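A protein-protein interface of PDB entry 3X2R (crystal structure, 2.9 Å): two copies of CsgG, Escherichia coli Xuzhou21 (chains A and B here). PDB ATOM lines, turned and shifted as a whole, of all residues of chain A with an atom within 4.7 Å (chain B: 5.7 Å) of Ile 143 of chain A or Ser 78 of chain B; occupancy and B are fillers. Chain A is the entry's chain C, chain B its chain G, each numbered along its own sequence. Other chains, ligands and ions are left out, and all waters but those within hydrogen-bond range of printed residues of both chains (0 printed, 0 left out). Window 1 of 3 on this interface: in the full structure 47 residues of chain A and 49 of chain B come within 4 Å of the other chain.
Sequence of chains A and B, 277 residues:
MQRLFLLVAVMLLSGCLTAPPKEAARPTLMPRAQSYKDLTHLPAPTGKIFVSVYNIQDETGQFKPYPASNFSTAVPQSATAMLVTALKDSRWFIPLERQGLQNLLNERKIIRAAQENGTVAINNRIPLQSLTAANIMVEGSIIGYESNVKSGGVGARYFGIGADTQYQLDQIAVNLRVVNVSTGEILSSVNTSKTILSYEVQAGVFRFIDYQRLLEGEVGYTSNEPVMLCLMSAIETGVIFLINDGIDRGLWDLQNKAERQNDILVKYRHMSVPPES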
ATOM      1  N   GLU A  59      18.218  15.117 -20.937  1.00  0.00           N
ATOM      2  CA  GLU A  59      19.242  15.005 -19.908  1.00  0.00           C
ATOM      3  C   GLU A  59      18.844  14.049 -18.779  1.00  0.00           C
ATOM      4  O   GLU A  59      19.427  14.082 -17.698  1.00  0.00           O
ATOM      5  CB  GLU A  59      19.676  16.379 -19.410  1.00  0.00           C
ATOM      6  CG  GLU A  59      20.268  17.224 -20.534  1.00  0.00           C
ATOM      7  CD  GLU A  59      20.570  18.658 -20.121  1.00  0.00           C
ATOM      8  OE1 GLU A  59      20.320  19.022 -18.947  1.00  0.00           O
ATOM      9  OE2 GLU A  59      21.048  19.424 -20.987  1.00  0.00           O
ATOM     10  N   THR A  60      17.766  13.298 -18.991  1.00  0.00           N
ATOM     11  CA  THR A  60      17.326  12.300 -18.016  1.00  0.00           C
ATOM     12  C   THR A  60      18.254  11.073 -17.898  1.00  0.00           C
ATOM     13  O   THR A  60      18.294  10.421 -16.851  1.00  0.00           O
ATOM     14  CB  THR A  60      15.883  11.836 -18.306  1.00  0.00           C
ATOM     15  OG1 THR A  60      15.191  11.596 -17.079  1.00  0.00           O
ATOM     16  CG2 THR A  60      15.875  10.570 -19.141  1.00  0.00           C
ATOM     17  N   SER A 141      15.754  21.580 -21.148  1.00  0.00           N
ATOM     18  CA  SER A 141      15.877  20.160 -21.411  1.00  0.00           C
ATOM     19  C   SER A 141      14.943  19.374 -20.514  1.00  0.00           C
ATOM     20  O   SER A 141      14.236  19.941 -19.677  1.00  0.00           O
ATOM     21  CB  SER A 141      17.313  19.713 -21.130  1.00  0.00           C
ATOM     22  OG  SER A 141      17.902  20.484 -20.092  1.00  0.00           O
ATOM     23  N   ILE A 142      14.956  18.058 -20.683  1.00  0.00           N
ATOM     24  CA  ILE A 142      14.200  17.190 -19.801  1.00  0.00           C
ATOM     25  C   ILE A 142      15.116  16.769 -18.660  1.00  0.00           C
ATOM     26  O   ILE A 142      16.058  15.987 -18.832  1.00  0.00           O
ATOM     27  CB  ILE A 142      13.677  15.974 -20.546  1.00  0.00           C
ATOM     28  CG1 ILE A 142      13.134  16.414 -21.905  1.00  0.00           C
ATOM     29  CG2 ILE A 142      12.640  15.245 -19.704  1.00  0.00           C
ATOM     30  CD1 ILE A 142      12.561  15.301 -22.740  1.00  0.00           C
ATOM     31  N   ILE A 143      14.788  17.297 -17.488  1.00  0.00           N
ATOM     32  CA  ILE A 143      15.626  17.267 -16.303  1.00  0.00           C
ATOM     33  C   ILE A 143      15.745  15.903 -15.641  1.00  0.00           C
ATOM     34  O   ILE A 143      16.816  15.528 -15.181  1.00  0.00           O
ATOM     35  CB  ILE A 143      15.113  18.321 -15.277  1.00  0.00           C
ATOM     36  CG1 ILE A 143      15.851  19.646 -15.438  1.00  0.00           C
ATOM     37  CG2 ILE A 143      15.217  17.831 -13.833  1.00  0.00           C
ATOM     38  CD1 ILE A 143      15.496  20.624 -14.340  1.00  0.00           C
ATOM     39  N   GLY A 144      14.655  15.154 -15.585  1.00  0.00           N
ATOM     40  CA  GLY A 144      14.679  13.906 -14.850  1.00  0.00           C
ATOM     41  C   GLY A 144      13.474  13.023 -15.052  1.00  0.00           C
ATOM     42  O   GLY A 144      12.423  13.476 -15.488  1.00  0.00           O
ATOM     43  N   ALA A 173      10.440  15.667 -15.091  1.00  0.00           N
ATOM     44  CA  ALA A 173      10.659  17.074 -14.839  1.00  0.00           C
ATOM     45  C   ALA A 173      11.256  17.720 -16.059  1.00  0.00           C
ATOM     46  O   ALA A 173      11.992  17.091 -16.813  1.00  0.00           O
ATOM     47  CB  ALA A 173      11.552  17.278 -13.647  1.00  0.00           C
ATOM     48  N   VAL A 174      10.945  18.995 -16.235  1.00  0.00           N
ATOM     49  CA  VAL A 174      11.349  19.741 -17.406  1.00  0.00           C
ATOM     50  C   VAL A 174      11.882  21.088 -16.970  1.00  0.00           C
ATOM     51  O   VAL A 174      11.394  21.673 -16.003  1.00  0.00           O
ATOM     52  CB  VAL A 174      10.147  19.969 -18.323  1.00  0.00           C
ATOM     53  CG1 VAL A 174      10.527  20.860 -19.500  1.00  0.00           C
ATOM     54  CG2 VAL A 174       9.608  18.638 -18.800  1.00  0.00           C
ATOM     55  N   ASN A 175      12.880  21.581 -17.688  1.00  0.00           N
ATOM     56  CA  ASN A 175      13.398  22.913 -17.451  1.00  0.00           C
ATOM     57  C   ASN A 175      13.337  23.735 -18.722  1.00  0.00           C
ATOM     58  O   ASN A 175      13.804  23.297 -19.784  1.00  0.00           O
ATOM     59  CB  ASN A 175      14.838  22.846 -16.960  1.00  0.00           C
ATOM     60  CG  ASN A 175      15.475  24.208 -16.853  1.00  0.00           C
ATOM     61  OD1 ASN A 175      16.186  24.648 -17.757  1.00  0.00           O
ATOM     62  ND2 ASN A 175      15.225  24.886 -15.747  1.00  0.00           N
ATOM     63  N   ASN A 191      11.398  25.107 -13.574  1.00  0.00           N
ATOM     64  CA  ASN A 191      11.361  23.660 -13.504  1.00  0.00           C
ATOM     65  C   ASN A 191       9.931  23.258 -13.198  1.00  0.00           C
ATOM     66  O   ASN A 191       9.346  23.714 -12.217  1.00  0.00           O
ATOM     67  CB  ASN A 191      12.305  23.131 -12.422  1.00  0.00           C
ATOM     68  CG  ASN A 191      13.768  23.407 -12.731  1.00  0.00           C
ATOM     69  OD1 ASN A 191      14.167  23.491 -13.895  1.00  0.00           O
ATOM     70  ND2 ASN A 191      14.569  23.572 -11.688  1.00  0.00           N
ATOM     71  N   PRO B  76      20.588  11.975 -12.519  1.00  0.00           N
ATOM     72  CA  PRO B  76      20.212  12.856 -13.634  1.00  0.00           C
ATOM     73  C   PRO B  76      21.418  13.497 -14.333  1.00  0.00           C
ATOM     74  O   PRO B  76      22.457  13.701 -13.708  1.00  0.00           O
ATOM     75  CB  PRO B  76      19.391  13.946 -12.946  1.00  0.00           C
ATOM     76  CG  PRO B  76      18.878  13.299 -11.702  1.00  0.00           C
ATOM     77  CD  PRO B  76      19.963  12.391 -11.250  1.00  0.00           C
ATOM     78  N   GLN B  77      21.288  13.776 -15.627  1.00  0.00           N
ATOM     79  CA  GLN B  77      22.343  14.447 -16.383  1.00  0.00           C
ATOM     80  C   GLN B  77      22.087  15.940 -16.430  1.00  0.00           C
ATOM     81  O   GLN B  77      22.771  16.683 -17.137  1.00  0.00           O
ATOM     82  CB  GLN B  77      22.426  13.899 -17.803  1.00  0.00           C
ATOM     83  CG  GLN B  77      23.657  13.058 -18.070  1.00  0.00           C
ATOM     84  CD  GLN B  77      23.829  11.939 -17.065  1.00  0.00           C
ATOM     85  OE1 GLN B  77      22.858  11.318 -16.634  1.00  0.00           O
ATOM     86  NE2 GLN B  77      25.069  11.678 -16.683  1.00  0.00           N
ATOM     87  N   SER B  78      21.067  16.358 -15.688  1.00  0.00           N
ATOM     88  CA  SER B  78      20.449  17.671 -15.856  1.00  0.00           C
ATOM     89  C   SER B  78      21.070  18.889 -15.184  1.00  0.00           C
ATOM     90  O   SER B  78      20.672  20.000 -15.494  1.00  0.00           O
ATOM     91  CB  SER B  78      18.992  17.593 -15.431  1.00  0.00           C
ATOM     92  OG  SER B  78      18.829  16.685 -14.359  1.00  0.00           O
ATOM     93  N   ALA B  79      22.034  18.714 -14.287  1.00  0.00           N
ATOM     94  CA  ALA B  79      22.630  19.880 -13.630  1.00  0.00           C
ATOM     95  C   ALA B  79      23.332  20.746 -14.680  1.00  0.00           C
ATOM     96  O   ALA B  79      23.643  20.266 -15.779  1.00  0.00           O
ATOM     97  CB  ALA B  79      23.572  19.463 -12.527  1.00  0.00           C
ATOM     98  N   THR B  80      23.605  21.999 -14.313  1.00  0.00           N
ATOM     99  CA  THR B  80      23.719  23.162 -15.214  1.00  0.00           C
ATOM    100  C   THR B  80      22.346  23.509 -15.754  1.00  0.00           C
ATOM    101  O   THR B  80      22.212  24.187 -16.776  1.00  0.00           O
ATOM    102  CB  THR B  80      24.618  22.932 -16.474  1.00  0.00           C
ATOM    103  OG1 THR B  80      25.458  21.781 -16.316  1.00  0.00           O
ATOM    104  CG2 THR B  80      25.445  24.164 -16.789  1.00  0.00           C
ATOM    105  N   ALA B  81      21.323  23.027 -15.062  1.00  0.00           N
ATOM    106  CA  ALA B  81      19.957  23.489 -15.246  1.00  0.00           C
ATOM    107  C   ALA B  81      19.446  23.718 -13.847  1.00  0.00           C
ATOM    108  O   ALA B  81      19.019  24.815 -13.506  1.00  0.00           O
ATOM    109  CB  ALA B  81      19.108  22.475 -15.976  1.00  0.00           C
ATOM    110  N   MET B  82      19.452  22.639 -13.066  1.00  0.00           N
ATOM    111  CA  MET B  82      19.136  22.687 -11.644  1.00  0.00           C
ATOM    112  C   MET B  82      19.895  23.814 -10.937  1.00  0.00           C
ATOM    113  O   MET B  82      19.318  24.593 -10.169  1.00  0.00           O
ATOM    114  CB  MET B  82      19.499  21.352 -10.985  1.00  0.00           C
ATOM    115  CG  MET B  82      18.833  20.123 -11.589  1.00  0.00           C
ATOM    116  SD  MET B  82      18.772  18.775 -10.382  1.00  0.00           S
ATOM    117  CE  MET B  82      17.691  17.612 -11.211  1.00  0.00           C
ATOM    118  N   MET B 228      16.339  12.782  -8.502  1.00  0.00           N
ATOM    119  CA  MET B 228      16.450  14.096  -9.126  1.00  0.00           C
ATOM    120  C   MET B 228      16.140  15.252  -8.157  1.00  0.00           C
ATOM    121  O   MET B 228      16.839  16.274  -8.140  1.00  0.00           O
ATOM    122  CB  MET B 228      15.538  14.143 -10.352  1.00  0.00           C
ATOM    123  CG  MET B 228      14.710  15.401 -10.481  1.00  0.00           C
ATOM    124  SD  MET B 228      13.561  15.229 -11.846  1.00  0.00           S
ATOM    125  CE  MET B 228      12.627  13.784 -11.344  1.00  0.00           C
ATOM    126  N   LEU B 231      18.921  15.613  -5.753  1.00  0.00           N
ATOM    127  CA  LEU B 231      20.005  16.302  -6.439  1.00  0.00           C
ATOM    128  C   LEU B 231      19.730  17.798  -6.342  1.00  0.00           C
ATOM    129  O   LEU B 231      20.622  18.593  -6.035  1.00  0.00           O
ATOM    130  CB  LEU B 231      20.060  15.885  -7.909  1.00  0.00           C
ATOM    131  CG  LEU B 231      21.377  15.986  -8.688  1.00  0.00           C
ATOM    132  CD1 LEU B 231      21.130  15.687 -10.162  1.00  0.00           C
ATOM    133  CD2 LEU B 231      22.083  17.314  -8.550  1.00  0.00           C
ATOM    134  N   MET B 232      18.486  18.176  -6.613  1.00  0.00           N
ATOM    135  CA  MET B 232      18.090  19.578  -6.535  1.00  0.00           C
ATOM    136  C   MET B 232      18.351  20.124  -5.127  1.00  0.00           C
ATOM    137  O   MET B 232      18.861  21.233  -4.957  1.00  0.00           O
ATOM    138  CB  MET B 232      16.615  19.738  -6.891  1.00  0.00           C
ATOM    139  CG  MET B 232      16.168  21.179  -6.978  1.00  0.00           C
ATOM    140  SD  MET B 232      16.833  21.972  -8.456  1.00  0.00           S
ATOM    141  CE  MET B 232      15.822  21.179  -9.710  1.00  0.00           C
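The backbone carbonyl oxygen (O) of Glu 59 of chain A is in hydrogen-bond range of the backbone NH (N) of Gln 77 of chain B (2.8 Å).
The backbone carbonyl oxygen (O) of Glu 59 of chain A lies within hydrogen-bond range of the backbone NH (N) of Ser 78 of chain B (3.5 Å).
O of Ile 143 of chain A sits at hydrogen-bond distance from OG of Ser 78 of chain B (2.5 Å).
OG of Ser 141 of chain A sits at hydrogen-bond distance from OE1 of Glu 59 of chain A, at 3.0 Å.
The backbone NH of Glu 59 of chain A lies within hydrogen-bond range of the backbone carbonyl oxygen of Ile 142 of chain A (3.1 Å).
The backbone NH (N) of Ile 143 of chain A lies within hydrogen-bond range of the backbone carbonyl oxygen (O) of Ala 173 of chain A.
The backbone NH (N) of Ala 173 of chain A sits at hydrogen-bond distance from the backbone carbonyl oxygen (O) of Gly 144 of chain A (3.0 Å).
ND2 of Asn 175 of chain A lies within hydrogen-bond range of OD1 of Asn 191 of chain A (2.5 Å).
Glu 59 of chain A touches Pro 76 of chain B.
O of Ile 143 of chain A touches CB of Pro 76 of chain B, 3.8 Å away.
CG2 of Ile 143 of chain A touches CE of Met 82 of chain B (3.6 Å).
SD of Met 228 of chain B touches CG2 of Ile 143 of chain A, at 3.7 Å.
CA of Gly 144 of chain A touches SD of Met 228 of chain B, 3.5 Å away.
Ala 173 of chain A touches Met 228 of chain B.
ND2 of Asn 191 of chain A touches CE of Met 232 of chain B, at 3.3 Å.
Of chain B, only Pro 76, Ser 78, Met 82 and Met 228 come within 4 Å of Ile 143 of chain A.
Ser 78 of chain B touches just these residues of chain A: Glu 59 and Ile 143.
Of the printed residues of chain A, Gln 77 of chain B touches Glu 59 (2.8 Å).
Printed residues of chain A within 4 Å of Met 228 of chain B: Ile 143, Gly 144 and Ala 173.
Of the printed residues of chain A, Met 82 of chain B touches Ile 143 (3.6 Å).
The nearest residue of chain B that does not touch Ile 143 of chain A is Ala 81 of chain B (4.3 Å).
Of the 10 printed residues of chain B, 6 touch a printed residue of chain A.
Hydrophobic or aromatic side chains of chain B within 4 Å of the printed part of chain A: Pro 76, Met 82, Met 228 and Met 232.
Hydrophobic or aromatic side chains of chain A that line the printed part of chain B: Ile 143 and Ala 173.
Among the printed residues, no Asp or Glu carboxylate lies within 4 Å of a Lys or Arg side-chain nitrogen of the other chain.
No position is printed for both chains.
Of the 10 pairs that touch across the chains among the printed residues, none has its exchanged pair printed and touching as well.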
